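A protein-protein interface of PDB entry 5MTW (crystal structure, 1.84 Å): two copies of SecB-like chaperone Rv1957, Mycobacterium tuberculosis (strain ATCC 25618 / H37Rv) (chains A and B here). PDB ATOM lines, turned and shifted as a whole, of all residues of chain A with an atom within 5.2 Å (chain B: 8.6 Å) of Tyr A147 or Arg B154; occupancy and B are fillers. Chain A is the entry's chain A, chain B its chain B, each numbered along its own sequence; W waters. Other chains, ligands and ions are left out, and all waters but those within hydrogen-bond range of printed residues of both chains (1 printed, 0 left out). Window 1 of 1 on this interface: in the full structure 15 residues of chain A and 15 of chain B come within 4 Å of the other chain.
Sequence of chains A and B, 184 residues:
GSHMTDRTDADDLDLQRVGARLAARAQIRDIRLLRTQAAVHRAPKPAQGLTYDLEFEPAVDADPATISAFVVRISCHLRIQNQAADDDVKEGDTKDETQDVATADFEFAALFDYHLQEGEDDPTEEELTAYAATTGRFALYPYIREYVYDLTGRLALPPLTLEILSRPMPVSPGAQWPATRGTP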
ATOM      1  N   ILE A  31      14.858  -7.434   4.261  1.00  0.00           N
ATOM      2  CA  ILE A  31      15.909  -6.553   3.729  1.00  0.00           C
ATOM      3  C   ILE A  31      16.948  -6.401   4.866  1.00  0.00           C
ATOM      4  O   ILE A  31      16.620  -6.490   6.043  1.00  0.00           O
ATOM      5  CB  ILE A  31      15.250  -5.216   3.290  1.00  0.00           C
ATOM      6  CG1 ILE A  31      14.545  -5.413   1.943  1.00  0.00           C
ATOM      7  CG2 ILE A  31      16.237  -4.095   3.064  1.00  0.00           C
ATOM      8  CD1 ILE A  31      13.366  -4.507   1.685  1.00  0.00           C
ATOM      9  N   ARG A  32      18.185  -6.131   4.527  1.00  0.00           N
ATOM     10  CA  ARG A  32      19.120  -5.649   5.510  1.00  0.00           C
ATOM     11  C   ARG A  32      20.126  -4.755   4.825  1.00  0.00           C
ATOM     12  O   ARG A  32      20.459  -4.898   3.602  1.00  0.00           O
ATOM     13  CB  ARG A  32      19.833  -6.798   6.190  1.00  0.00           C
ATOM     14  CG  ARG A  32      20.865  -7.500   5.314  1.00  0.00           C
ATOM     15  CD  ARG A  32      21.340  -8.810   5.964  1.00  0.00           C
ATOM     16  NE  ARG A  32      22.129  -9.637   5.039  1.00  0.00           N
ATOM     17  CZ  ARG A  32      23.105 -10.462   5.414  1.00  0.00           C
ATOM     18  NH1 ARG A  32      23.421 -10.540   6.688  1.00  0.00           N
ATOM     19  NH2 ARG A  32      23.780 -11.204   4.516  1.00  0.00           N
ATOM     20  N   LEU A  33      20.632  -3.840   5.628  1.00  0.00           N
ATOM     21  CA  LEU A  33      21.766  -3.066   5.279  1.00  0.00           C
ATOM     22  C   LEU A  33      22.975  -3.974   5.409  1.00  0.00           C
ATOM     23  O   LEU A  33      23.111  -4.624   6.385  1.00  0.00           O
ATOM     24  CB  LEU A  33      21.879  -1.841   6.234  1.00  0.00           C
ATOM     25  CG  LEU A  33      23.163  -0.998   6.125  1.00  0.00           C
ATOM     26  CD1 LEU A  33      23.097  -0.189   4.842  1.00  0.00           C
ATOM     27  CD2 LEU A  33      23.319  -0.034   7.301  1.00  0.00           C
ATOM     28  N   THR A  36      27.831   0.328   5.296  1.00  0.00           N
ATOM     29  CA  THR A  36      27.641   1.753   5.046  1.00  0.00           C
ATOM     30  C   THR A  36      28.921   2.544   5.384  1.00  0.00           C
ATOM     31  O   THR A  36      29.736   2.057   6.118  1.00  0.00           O
ATOM     32  CB  THR A  36      26.408   2.318   5.851  1.00  0.00           C
ATOM     33  OG1 THR A  36      26.195   3.617   5.391  1.00  0.00           O
ATOM     34  CG2 THR A  36      26.710   2.407   7.299  1.00  0.00           C
ATOM     35  N   PHE A 106      26.954   2.769   0.463  1.00  0.00           N
ATOM     36  CA  PHE A 106      26.252   1.758   1.212  1.00  0.00           C
ATOM     37  C   PHE A 106      25.605   0.702   0.278  1.00  0.00           C
ATOM     38  O   PHE A 106      25.502   0.924  -0.922  1.00  0.00           O
ATOM     39  CB  PHE A 106      25.164   2.392   2.091  1.00  0.00           C
ATOM     40  CG  PHE A 106      24.146   3.196   1.345  1.00  0.00           C
ATOM     41  CD1 PHE A 106      24.316   4.548   1.099  1.00  0.00           C
ATOM     42  CD2 PHE A 106      22.930   2.640   1.044  1.00  0.00           C
ATOM     43  CE1 PHE A 106      23.339   5.287   0.484  1.00  0.00           C
ATOM     44  CE2 PHE A 106      21.949   3.381   0.434  1.00  0.00           C
ATOM     45  CZ  PHE A 106      22.164   4.689   0.105  1.00  0.00           C
ATOM     46  N   PHE A 108      22.520  -2.493   0.200  1.00  0.00           N
ATOM     47  CA  PHE A 108      21.379  -3.145   0.811  1.00  0.00           C
ATOM     48  C   PHE A 108      21.219  -4.506   0.132  1.00  0.00           C
ATOM     49  O   PHE A 108      21.659  -4.675  -0.977  1.00  0.00           O
ATOM     50  CB  PHE A 108      20.131  -2.354   0.598  1.00  0.00           C
ATOM     51  CG  PHE A 108      19.917  -1.299   1.654  1.00  0.00           C
ATOM     52  CD1 PHE A 108      20.450  -0.034   1.495  1.00  0.00           C
ATOM     53  CD2 PHE A 108      19.251  -1.613   2.828  1.00  0.00           C
ATOM     54  CE1 PHE A 108      20.277   0.922   2.477  1.00  0.00           C
ATOM     55  CE2 PHE A 108      19.021  -0.647   3.819  1.00  0.00           C
ATOM     56  CZ  PHE A 108      19.572   0.627   3.654  1.00  0.00           C
ATOM     57  N   TYR A 143      12.995   1.664   0.912  1.00  0.00           N
ATOM     58  CA  TYR A 143      13.771   1.416   2.124  1.00  0.00           C
ATOM     59  C   TYR A 143      15.050   2.211   2.020  1.00  0.00           C
ATOM     60  O   TYR A 143      15.536   2.771   2.994  1.00  0.00           O
ATOM     61  CB  TYR A 143      14.000  -0.085   2.440  1.00  0.00           C
ATOM     62  CG  TYR A 143      12.709  -0.761   2.700  1.00  0.00           C
ATOM     63  CD1 TYR A 143      11.872  -1.227   1.674  1.00  0.00           C
ATOM     64  CD2 TYR A 143      12.261  -0.886   3.991  1.00  0.00           C
ATOM     65  CE1 TYR A 143      10.597  -1.791   1.998  1.00  0.00           C
ATOM     66  CE2 TYR A 143      11.049  -1.451   4.271  1.00  0.00           C
ATOM     67  CZ  TYR A 143      10.221  -1.903   3.281  1.00  0.00           C
ATOM     68  OH  TYR A 143       8.998  -2.452   3.686  1.00  0.00           O
ATOM     69  N   ILE A 144      15.601   2.290   0.825  1.00  0.00           N
ATOM     70  CA  ILE A 144      16.767   3.126   0.603  1.00  0.00           C
ATOM     71  C   ILE A 144      16.415   4.583   0.908  1.00  0.00           C
ATOM     72  O   ILE A 144      17.158   5.298   1.607  1.00  0.00           O
ATOM     73  CB  ILE A 144      17.362   2.915  -0.838  1.00  0.00           C
ATOM     74  CG1 ILE A 144      17.781   1.447  -1.012  1.00  0.00           C
ATOM     75  CG2 ILE A 144      18.383   3.939  -1.109  1.00  0.00           C
ATOM     76  CD1 ILE A 144      18.223   1.051  -2.415  1.00  0.00           C
ATOM     77  N   ARG A 145      15.230   5.006   0.472  1.00  0.00           N
ATOM     78  CA  ARG A 145      14.793   6.348   0.689  1.00  0.00           C
ATOM     79  C   ARG A 145      14.788   6.597   2.240  1.00  0.00           C
ATOM     80  O   ARG A 145      15.348   7.610   2.762  1.00  0.00           O
ATOM     81  CB  ARG A 145      13.415   6.577   0.097  1.00  0.00           C
ATOM     82  CG  ARG A 145      12.903   7.978   0.447  1.00  0.00           C
ATOM     83  CD  ARG A 145      11.533   8.308  -0.031  1.00  0.00           C
ATOM     84  NE  ARG A 145      11.478   8.413  -1.512  1.00  0.00           N
ATOM     85  CZ  ARG A 145      10.876   7.542  -2.330  1.00  0.00           C
ATOM     86  NH1 ARG A 145      10.222   6.483  -1.858  1.00  0.00           N
ATOM     87  NH2 ARG A 145      10.988   7.712  -3.645  1.00  0.00           N
ATOM     88  N   GLU A 146      14.177   5.677   2.972  1.00  0.00           N
ATOM     89  CA  GLU A 146      14.028   5.930   4.451  1.00  0.00           C
ATOM     90  C   GLU A 146      15.440   5.959   5.120  1.00  0.00           C
ATOM     91  O   GLU A 146      15.762   6.751   5.909  1.00  0.00           O
ATOM     92  CB  GLU A 146      13.209   4.798   5.052  1.00  0.00           C
ATOM     93  CG  GLU A 146      12.922   5.038   6.554  1.00  0.00           C
ATOM     94  CD  GLU A 146      14.004   4.558   7.459  1.00  0.00           C
ATOM     95  OE1 GLU A 146      14.560   3.507   7.073  1.00  0.00           O
ATOM     96  OE2 GLU A 146      14.265   5.199   8.534  1.00  0.00           O
ATOM     97  N   TYR A 147      16.314   5.115   4.648  1.00  0.00           N
ATOM     98  CA  TYR A 147      17.670   5.105   5.171  1.00  0.00           C
ATOM     99  C   TYR A 147      18.427   6.413   4.925  1.00  0.00           C
ATOM    100  O   TYR A 147      19.080   6.943   5.848  1.00  0.00           O
ATOM    101  CB  TYR A 147      18.463   3.919   4.630  1.00  0.00           C
ATOM    102  CG  TYR A 147      19.873   3.969   5.191  1.00  0.00           C
ATOM    103  CD1 TYR A 147      20.131   3.749   6.535  1.00  0.00           C
ATOM    104  CD2 TYR A 147      20.932   4.243   4.359  1.00  0.00           C
ATOM    105  CE1 TYR A 147      21.454   3.753   7.044  1.00  0.00           C
ATOM    106  CE2 TYR A 147      22.220   4.286   4.861  1.00  0.00           C
ATOM    107  CZ  TYR A 147      22.497   4.026   6.171  1.00  0.00           C
ATOM    108  OH  TYR A 147      23.896   4.101   6.576  1.00  0.00           O
ATOM    109  N   VAL A 148      18.317   6.934   3.693  1.00  0.00           N
ATOM    110  CA  VAL A 148      18.962   8.147   3.317  1.00  0.00           C
ATOM    111  C   VAL A 148      18.419   9.310   4.107  1.00  0.00           C
ATOM    112  O   VAL A 148      19.197  10.162   4.573  1.00  0.00           O
ATOM    113  CB  VAL A 148      18.869   8.408   1.762  1.00  0.00           C
ATOM    114  CG1 VAL A 148      19.315   9.847   1.346  1.00  0.00           C
ATOM    115  CG2 VAL A 148      19.622   7.303   1.024  1.00  0.00           C
ATOM    116  N   TYR A 149      17.093   9.318   4.291  1.00  0.00           N
ATOM    117  CA  TYR A 149      16.457  10.386   5.048  1.00  0.00           C
ATOM    118  C   TYR A 149      16.964  10.374   6.505  1.00  0.00           C
ATOM    119  O   TYR A 149      17.314  11.398   7.105  1.00  0.00           O
ATOM    120  CB  TYR A 149      14.960  10.089   4.954  1.00  0.00           C
ATOM    121  CG  TYR A 149      14.050  10.957   5.745  1.00  0.00           C
ATOM    122  CD1 TYR A 149      13.850  10.706   7.062  1.00  0.00           C
ATOM    123  CD2 TYR A 149      13.319  11.965   5.138  1.00  0.00           C
ATOM    124  CE1 TYR A 149      12.927  11.491   7.806  1.00  0.00           C
ATOM    125  CE2 TYR A 149      12.390  12.729   5.827  1.00  0.00           C
ATOM    126  CZ  TYR A 149      12.246  12.544   7.188  1.00  0.00           C
ATOM    127  OH  TYR A 149      11.276  13.256   7.888  1.00  0.00           O
ATOM    128  N   ASP A 150      17.021   9.192   7.096  1.00  0.00           N
ATOM    129  CA  ASP A 150      17.525   9.048   8.439  1.00  0.00           C
ATOM    130  C   ASP A 150      18.992   9.452   8.574  1.00  0.00           C
ATOM    131  O   ASP A 150      19.389  10.180   9.499  1.00  0.00           O
ATOM    132  CB  ASP A 150      17.409   7.588   8.899  1.00  0.00           C
ATOM    133  CG  ASP A 150      17.947   7.384  10.339  1.00  0.00           C
ATOM    134  OD1 ASP A 150      17.277   7.883  11.235  1.00  0.00           O
ATOM    135  OD2 ASP A 150      19.060   6.851  10.539  1.00  0.00           O
ATOM    136  N   LEU A 151      19.812   8.950   7.653  1.00  0.00           N
ATOM    137  CA  LEU A 151      21.241   9.269   7.684  1.00  0.00           C
ATOM    138  C   LEU A 151      21.563  10.776   7.535  1.00  0.00           C
ATOM    139  O   LEU A 151      22.375  11.341   8.260  1.00  0.00           O
ATOM    140  CB  LEU A 151      21.975   8.508   6.607  1.00  0.00           C
ATOM    141  CG  LEU A 151      23.475   8.735   6.485  1.00  0.00           C
ATOM    142  CD1 LEU A 151      24.231   8.139   7.693  1.00  0.00           C
ATOM    143  CD2 LEU A 151      23.989   8.102   5.197  1.00  0.00           C
ATOM    144  N   THR A 152      21.006  11.381   6.502  1.00  0.00           N
ATOM    145  CA  THR A 152      21.165  12.863   6.294  1.00  0.00           C
ATOM    146  C   THR A 152      20.678  13.694   7.487  1.00  0.00           C
ATOM    147  O   THR A 152      21.395  14.643   7.824  1.00  0.00           O
ATOM    148  CB  THR A 152      20.552  13.369   4.955  1.00  0.00           C
ATOM    149  OG1 THR A 152      19.157  13.055   4.954  1.00  0.00           O
ATOM    150  CG2 THR A 152      21.312  12.644   3.755  1.00  0.00           C
ATOM    151  N   LEU B  33      25.970  13.465  14.089  1.00  0.00           N
ATOM    152  CA  LEU B  33      26.855  12.434  13.629  1.00  0.00           C
ATOM    153  C   LEU B  33      27.795  13.095  12.641  1.00  0.00           C
ATOM    154  O   LEU B  33      27.288  13.802  11.793  1.00  0.00           O
ATOM    155  CB  LEU B  33      26.010  11.402  12.854  1.00  0.00           C
ATOM    156  CG  LEU B  33      26.794  10.214  12.240  1.00  0.00           C
ATOM    157  CD1 LEU B  33      27.282   9.371  13.392  1.00  0.00           C
ATOM    158  CD2 LEU B  33      25.947   9.394  11.318  1.00  0.00           C
ATOM    159  N   THR B  36      30.333   7.793   9.787  1.00  0.00           N
ATOM    160  CA  THR B  36      30.104   6.468  10.213  1.00  0.00           C
ATOM    161  C   THR B  36      30.614   5.465   9.154  1.00  0.00           C
ATOM    162  O   THR B  36      30.699   5.786   8.001  1.00  0.00           O
ATOM    163  CB  THR B  36      28.572   6.254  10.494  1.00  0.00           C
ATOM    164  OG1 THR B  36      28.354   4.972  11.101  1.00  0.00           O
ATOM    165  CG2 THR B  36      27.809   6.278   9.184  1.00  0.00           C
ATOM    166  N   GLN B  37      30.947   4.286   9.598  1.00  0.00           N
ATOM    167  CA  GLN B  37      31.277   3.119   8.724  1.00  0.00           C
ATOM    168  C   GLN B  37      30.816   1.888   9.454  1.00  0.00           C
ATOM    169  O   GLN B  37      30.991   1.819  10.671  1.00  0.00           O
ATOM    170  CB  GLN B  37      32.801   3.015   8.557  1.00  0.00           C
ATOM    171  CG  GLN B  37      33.272   1.932   7.605  1.00  0.00           C
ATOM    172  CD  GLN B  37      34.726   2.166   7.208  1.00  0.00           C
ATOM    173  OE1 GLN B  37      35.293   3.184   7.561  1.00  0.00           O
ATOM    174  NE2 GLN B  37      35.315   1.235   6.456  1.00  0.00           N
ATOM    175  N   ALA B  38      30.245   0.897   8.747  1.00  0.00           N
ATOM    176  CA  ALA B  38      29.763  -0.272   9.414  1.00  0.00           C
ATOM    177  C   ALA B  38      29.560  -1.358   8.409  1.00  0.00           C
ATOM    178  O   ALA B  38      29.396  -1.077   7.235  1.00  0.00           O
ATOM    179  CB  ALA B  38      28.461  -0.008  10.189  1.00  0.00           C
ATOM    180  N   VAL B  40      28.410  -5.868   8.143  1.00  0.00           N
ATOM    181  CA  VAL B  40      28.158  -7.187   8.687  1.00  0.00           C
ATOM    182  C   VAL B  40      29.069  -8.176   7.934  1.00  0.00           C
ATOM    183  O   VAL B  40      29.183  -8.115   6.750  1.00  0.00           O
ATOM    184  CB  VAL B  40      26.661  -7.576   8.742  1.00  0.00           C
ATOM    185  CG1 VAL B  40      25.982  -7.434   7.392  1.00  0.00           C
ATOM    186  CG2 VAL B  40      26.494  -8.977   9.273  1.00  0.00           C
ATOM    187  N   GLU B 146      21.444   5.106  21.117  1.00  0.00           N
ATOM    188  CA  GLU B 146      20.356   5.036  20.119  1.00  0.00           C
ATOM    189  C   GLU B 146      20.917   4.673  18.712  1.00  0.00           C
ATOM    190  O   GLU B 146      20.321   3.894  17.993  1.00  0.00           O
ATOM    191  CB  GLU B 146      19.467   6.302  20.177  1.00  0.00           C
ATOM    192  CG  GLU B 146      18.260   6.361  19.233  1.00  0.00           C
ATOM    193  CD  GLU B 146      18.605   6.526  17.773  1.00  0.00           C
ATOM    194  OE1 GLU B 146      19.632   7.142  17.448  1.00  0.00           O
ATOM    195  OE2 GLU B 146      17.877   5.988  16.924  1.00  0.00           O
ATOM    196  N   TYR B 147      22.051   5.233  18.369  1.00  0.00           N
ATOM    197  CA  TYR B 147      22.599   4.907  17.050  1.00  0.00           C
ATOM    198  C   TYR B 147      22.895   3.416  16.977  1.00  0.00           C
ATOM    199  O   TYR B 147      22.631   2.766  15.932  1.00  0.00           O
ATOM    200  CB  TYR B 147      23.864   5.709  16.796  1.00  0.00           C
ATOM    201  CG  TYR B 147      24.364   5.505  15.434  1.00  0.00           C
ATOM    202  CD1 TYR B 147      23.595   5.863  14.324  1.00  0.00           C
ATOM    203  CD2 TYR B 147      25.588   4.888  15.236  1.00  0.00           C
ATOM    204  CE1 TYR B 147      24.093   5.643  13.045  1.00  0.00           C
ATOM    205  CE2 TYR B 147      26.070   4.667  13.987  1.00  0.00           C
ATOM    206  CZ  TYR B 147      25.305   5.032  12.880  1.00  0.00           C
ATOM    207  OH  TYR B 147      25.765   4.773  11.595  1.00  0.00           O
ATOM    208  N   VAL B 148      23.534   2.902  18.054  1.00  0.00           N
ATOM    209  CA  VAL B 148      23.830   1.456  18.107  1.00  0.00           C
ATOM    210  C   VAL B 148      22.614   0.544  17.921  1.00  0.00           C
ATOM    211  O   VAL B 148      22.634  -0.409  17.105  1.00  0.00           O
ATOM    212  CB  VAL B 148      24.645   1.066  19.297  1.00  0.00           C
ATOM    213  CG1 VAL B 148      24.815  -0.448  19.351  1.00  0.00           C
ATOM    214  CG2 VAL B 148      25.988   1.693  19.095  1.00  0.00           C
ATOM    215  N   TYR B 149      21.572   0.918  18.640  1.00  0.00           N
ATOM    216  CA  TYR B 149      20.281   0.229  18.535  1.00  0.00           C
ATOM    217  C   TYR B 149      19.780   0.258  17.105  1.00  0.00           C
ATOM    218  O   TYR B 149      19.301  -0.763  16.594  1.00  0.00           O
ATOM    219  CB  TYR B 149      19.300   0.837  19.553  1.00  0.00           C
ATOM    220  CG  TYR B 149      17.873   0.253  19.487  1.00  0.00           C
ATOM    221  CD1 TYR B 149      17.576  -1.001  20.016  1.00  0.00           C
ATOM    222  CD2 TYR B 149      16.820   0.956  18.781  1.00  0.00           C
ATOM    223  CE1 TYR B 149      16.269  -1.508  19.931  1.00  0.00           C
ATOM    224  CE2 TYR B 149      15.538   0.452  18.685  1.00  0.00           C
ATOM    225  CZ  TYR B 149      15.257  -0.791  19.285  1.00  0.00           C
ATOM    226  OH  TYR B 149      14.015  -1.315  19.179  1.00  0.00           O
ATOM    227  N   ASP B 150      19.769   1.430  16.470  1.00  0.00           N
ATOM    228  CA  ASP B 150      19.197   1.566  15.123  1.00  0.00           C
ATOM    229  C   ASP B 150      20.037   0.794  14.125  1.00  0.00           C
ATOM    230  O   ASP B 150      19.539   0.149  13.193  1.00  0.00           O
ATOM    231  CB  ASP B 150      19.246   3.053  14.652  1.00  0.00           C
ATOM    232  CG  ASP B 150      18.717   3.246  13.196  1.00  0.00           C
ATOM    233  OD1 ASP B 150      17.478   3.159  13.026  1.00  0.00           O
ATOM    234  OD2 ASP B 150      19.495   3.447  12.241  1.00  0.00           O
ATOM    235  N   LEU B 151      21.337   0.911  14.324  1.00  0.00           N
ATOM    236  CA  LEU B 151      22.293   0.285  13.350  1.00  0.00           C
ATOM    237  C   LEU B 151      22.253  -1.268  13.313  1.00  0.00           C
ATOM    238  O   LEU B 151      22.175  -1.891  12.186  1.00  0.00           O
ATOM    239  CB  LEU B 151      23.698   0.778  13.643  1.00  0.00           C
ATOM    240  CG  LEU B 151      24.808   0.220  12.794  1.00  0.00           C
ATOM    241  CD1 LEU B 151      24.555   0.494  11.342  1.00  0.00           C
ATOM    242  CD2 LEU B 151      26.135   0.796  13.197  1.00  0.00           C
ATOM    243  N   THR B 152      22.264  -1.880  14.509  1.00  0.00           N
ATOM    244  CA  THR B 152      22.138  -3.327  14.623  1.00  0.00           C
ATOM    245  C   THR B 152      20.798  -3.787  13.987  1.00  0.00           C
ATOM    246  O   THR B 152      20.771  -4.814  13.310  1.00  0.00           O
ATOM    247  CB  THR B 152      22.275  -3.842  16.046  1.00  0.00           C
ATOM    248  OG1 THR B 152      21.465  -3.094  16.973  1.00  0.00           O
ATOM    249  CG2 THR B 152      23.715  -3.687  16.472  1.00  0.00           C
ATOM    250  N   GLY B 153      19.727  -3.021  14.197  1.00  0.00           N
ATOM    251  CA  GLY B 153      18.464  -3.326  13.518  1.00  0.00           C
ATOM    252  C   GLY B 153      18.547  -3.310  12.011  1.00  0.00           C
ATOM    253  O   GLY B 153      18.135  -4.269  11.366  1.00  0.00           O
ATOM    254  N   ARG B 154      19.139  -2.264  11.450  1.00  0.00           N
ATOM    255  CA  ARG B 154      19.254  -2.143  10.009  1.00  0.00           C
ATOM    256  C   ARG B 154      20.157  -3.215   9.438  1.00  0.00           C
ATOM    257  O   ARG B 154      19.910  -3.724   8.321  1.00  0.00           O
ATOM    258  CB  ARG B 154      19.808  -0.762   9.616  1.00  0.00           C
ATOM    259  CG  ARG B 154      18.792   0.357   9.956  1.00  0.00           C
ATOM    260  CD  ARG B 154      19.379   1.609   9.364  1.00  0.00           C
ATOM    261  NE  ARG B 154      18.596   2.748   9.783  1.00  0.00           N
ATOM    262  CZ  ARG B 154      17.482   3.156   9.216  1.00  0.00           C
ATOM    263  NH1 ARG B 154      17.027   2.583   8.139  1.00  0.00           N
ATOM    264  NH2 ARG B 154      16.842   4.179   9.718  1.00  0.00           N
ATOM    265  N   LEU B 155      21.175  -3.575  10.193  1.00  0.00           N
ATOM    266  CA  LEU B 155      22.013  -4.730   9.764  1.00  0.00           C
ATOM    267  C   LEU B 155      21.273  -6.130   9.918  1.00  0.00           C
ATOM    268  O   LEU B 155      21.843  -7.160   9.605  1.00  0.00           O
ATOM    269  CB  LEU B 155      23.334  -4.759  10.530  1.00  0.00           C
ATOM    270  CG  LEU B 155      24.261  -3.529  10.359  1.00  0.00           C
ATOM    271  CD1 LEU B 155      25.399  -3.523  11.384  1.00  0.00           C
ATOM    272  CD2 LEU B 155      24.761  -3.392   8.928  1.00  0.00           C
ATOM    273  N   ALA B 156      20.068  -6.164  10.462  1.00  0.00           N
ATOM    274  CA  ALA B 156      19.337  -7.404  10.732  1.00  0.00           C
ATOM    275  C   ALA B 156      20.044  -8.275  11.770  1.00  0.00           C
ATOM    276  O   ALA B 156      19.901  -9.458  11.769  1.00  0.00           O
ATOM    277  CB  ALA B 156      19.044  -8.200   9.444  1.00  0.00           C
ATOM    278  N   LEU B 157      20.750  -7.672  12.710  1.00  0.00           N
ATOM    279  CA  LEU B 157      21.294  -8.414  13.839  1.00  0.00           C
ATOM    280  C   LEU B 157      20.304  -8.370  14.996  1.00  0.00           C
ATOM    281  O   LEU B 157      19.411  -7.540  14.987  1.00  0.00           O
ATOM    282  CB  LEU B 157      22.595  -7.789  14.300  1.00  0.00           C
ATOM    283  CG  LEU B 157      23.654  -7.763  13.171  1.00  0.00           C
ATOM    284  CD1 LEU B 157      24.914  -7.084  13.676  1.00  0.00           C
ATOM    285  CD2 LEU B 157      23.933  -9.199  12.678  1.00  0.00           C
ATOM    286  N   PRO B 158      20.481  -9.239  16.015  1.00  0.00           N
ATOM    287  CA  PRO B 158      19.734  -8.981  17.223  1.00  0.00           C
ATOM    288  C   PRO B 158      19.996  -7.504  17.714  1.00  0.00           C
ATOM    289  O   PRO B 158      21.168  -7.002  17.782  1.00  0.00           O
ATOM    290  CB  PRO B 158      20.322 -10.014  18.218  1.00  0.00           C
ATOM    291  CG  PRO B 158      20.694 -11.136  17.366  1.00  0.00           C
ATOM    292  CD  PRO B 158      21.350 -10.428  16.192  1.00  0.00           C
ATOM    293  N   PRO B 159      18.921  -6.778  17.975  1.00  0.00           N
ATOM    294  CA  PRO B 159      19.131  -5.357  18.385  1.00  0.00           C
ATOM    295  C   PRO B 159      19.893  -5.243  19.697  1.00  0.00           C
ATOM    296  O   PRO B 159      19.554  -5.861  20.694  1.00  0.00           O
ATOM    297  CB  PRO B 159      17.672  -4.815  18.495  1.00  0.00           C
ATOM    298  CG  PRO B 159      16.917  -5.735  17.568  1.00  0.00           C
ATOM    299  CD  PRO B 159      17.475  -7.089  17.868  1.00  0.00           C
HETATM  300  O   HOH W   1      23.653   4.749   9.420  1.00  0.00           O
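The side-chain hydroxyl of Thr A36 sits at hydrogen-bond distance from the side-chain hydroxyl of Tyr A147 (2.6 Å).
The guanidinium group (NE) of Arg B154 is in salt-bridge range of the side-chain carboxylate (OD2) of Asp B150, 2.7 Å away.
Tyr A147 touches one residue of chain B.
Of chain A, only Arg A32 (3.5 Å), Leu A33 (2.8 Å), Glu A146 (2.8 Å), Tyr A147 (3.6 Å) and Asp A150 (3.4 Å) come within 4 Å of Arg B154.
Glu A146 touches one residue of chain B.
Of the printed residues of chain A, Ala B38 touches Thr A36 (2.9 Å).
Of the printed residues of chain B, Thr A36 touches Gln B37 (3.2 Å) and Ala B38 (2.9 Å).
Of the printed residues of chain A, Leu B155 touches Arg A32 (3.98 Å) and Leu A33 (3.3 Å).
Printed residues of chain B within 4 Å of Leu A33: Arg B154 (2.8 Å) and Leu B155 (3.3 Å).
Of the printed residues of chain B, Asp A150 touches Asp B150 (3.8 Å) and Arg B154 (3.4 Å).
Pro B159 touches none of the printed residues of chain A.
The nearest residue of chain B that does not touch Tyr A147 is Thr B36 (5.2 Å).
The nearest printed residue of chain A that does not touch Gln B37 is Tyr A147 (7.7 Å).
Among the printed residues, merely in contact across the chains: Arg A32 with Arg B154 (3.5 Å), Arg A32 with Leu B155 (3.98 Å), Arg A32 with Ala B156 (3.6 Å), Leu A33 with Leu B155 (3.3 Å), Thr A36 with Gln B37 (3.2 Å), Tyr A147 with Arg B154 (3.6 Å) and Asp A150 with Asp B150 (3.8 Å).
Water W1 lies within hydrogen-bond range of the side-chain hydroxyl of Tyr A147 (2.9 Å) and the side-chain hydroxyl of Tyr B147 (3.0 Å).
Hydrophobic or aromatic side chains of chain A that line the printed part of chain B: Leu A33 and Tyr A147.
Hydrophobic or aromatic side chains of chain B within 4 Å of the printed part of chain A: Leu B155 and Ala B156.
Among the printed residues, Asp or Glu carboxylates within 4 Å of a Lys or Arg side-chain nitrogen of the other chain: Glu A146 with Arg B154 and Asp A150 with Arg B154.
The backbone NH of Leu A33 sits at hydrogen-bond distance from the backbone carbonyl oxygen of Arg B154 (2.8 Å).
N of Thr A36 lies within hydrogen-bond range of O of Ala B38, 2.9 Å away.
The guanidinium group (NH1) of Arg B154 is in salt-bridge range of the side-chain carboxylate (OE1) of Glu A146 (2.8 Å).
The guanidinium group (NH2) of Arg B154 is in salt-bridge range of the side-chain carboxylate (OD2) of Asp A150.
Asp B150 touches its own counterpart, Asp A150.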
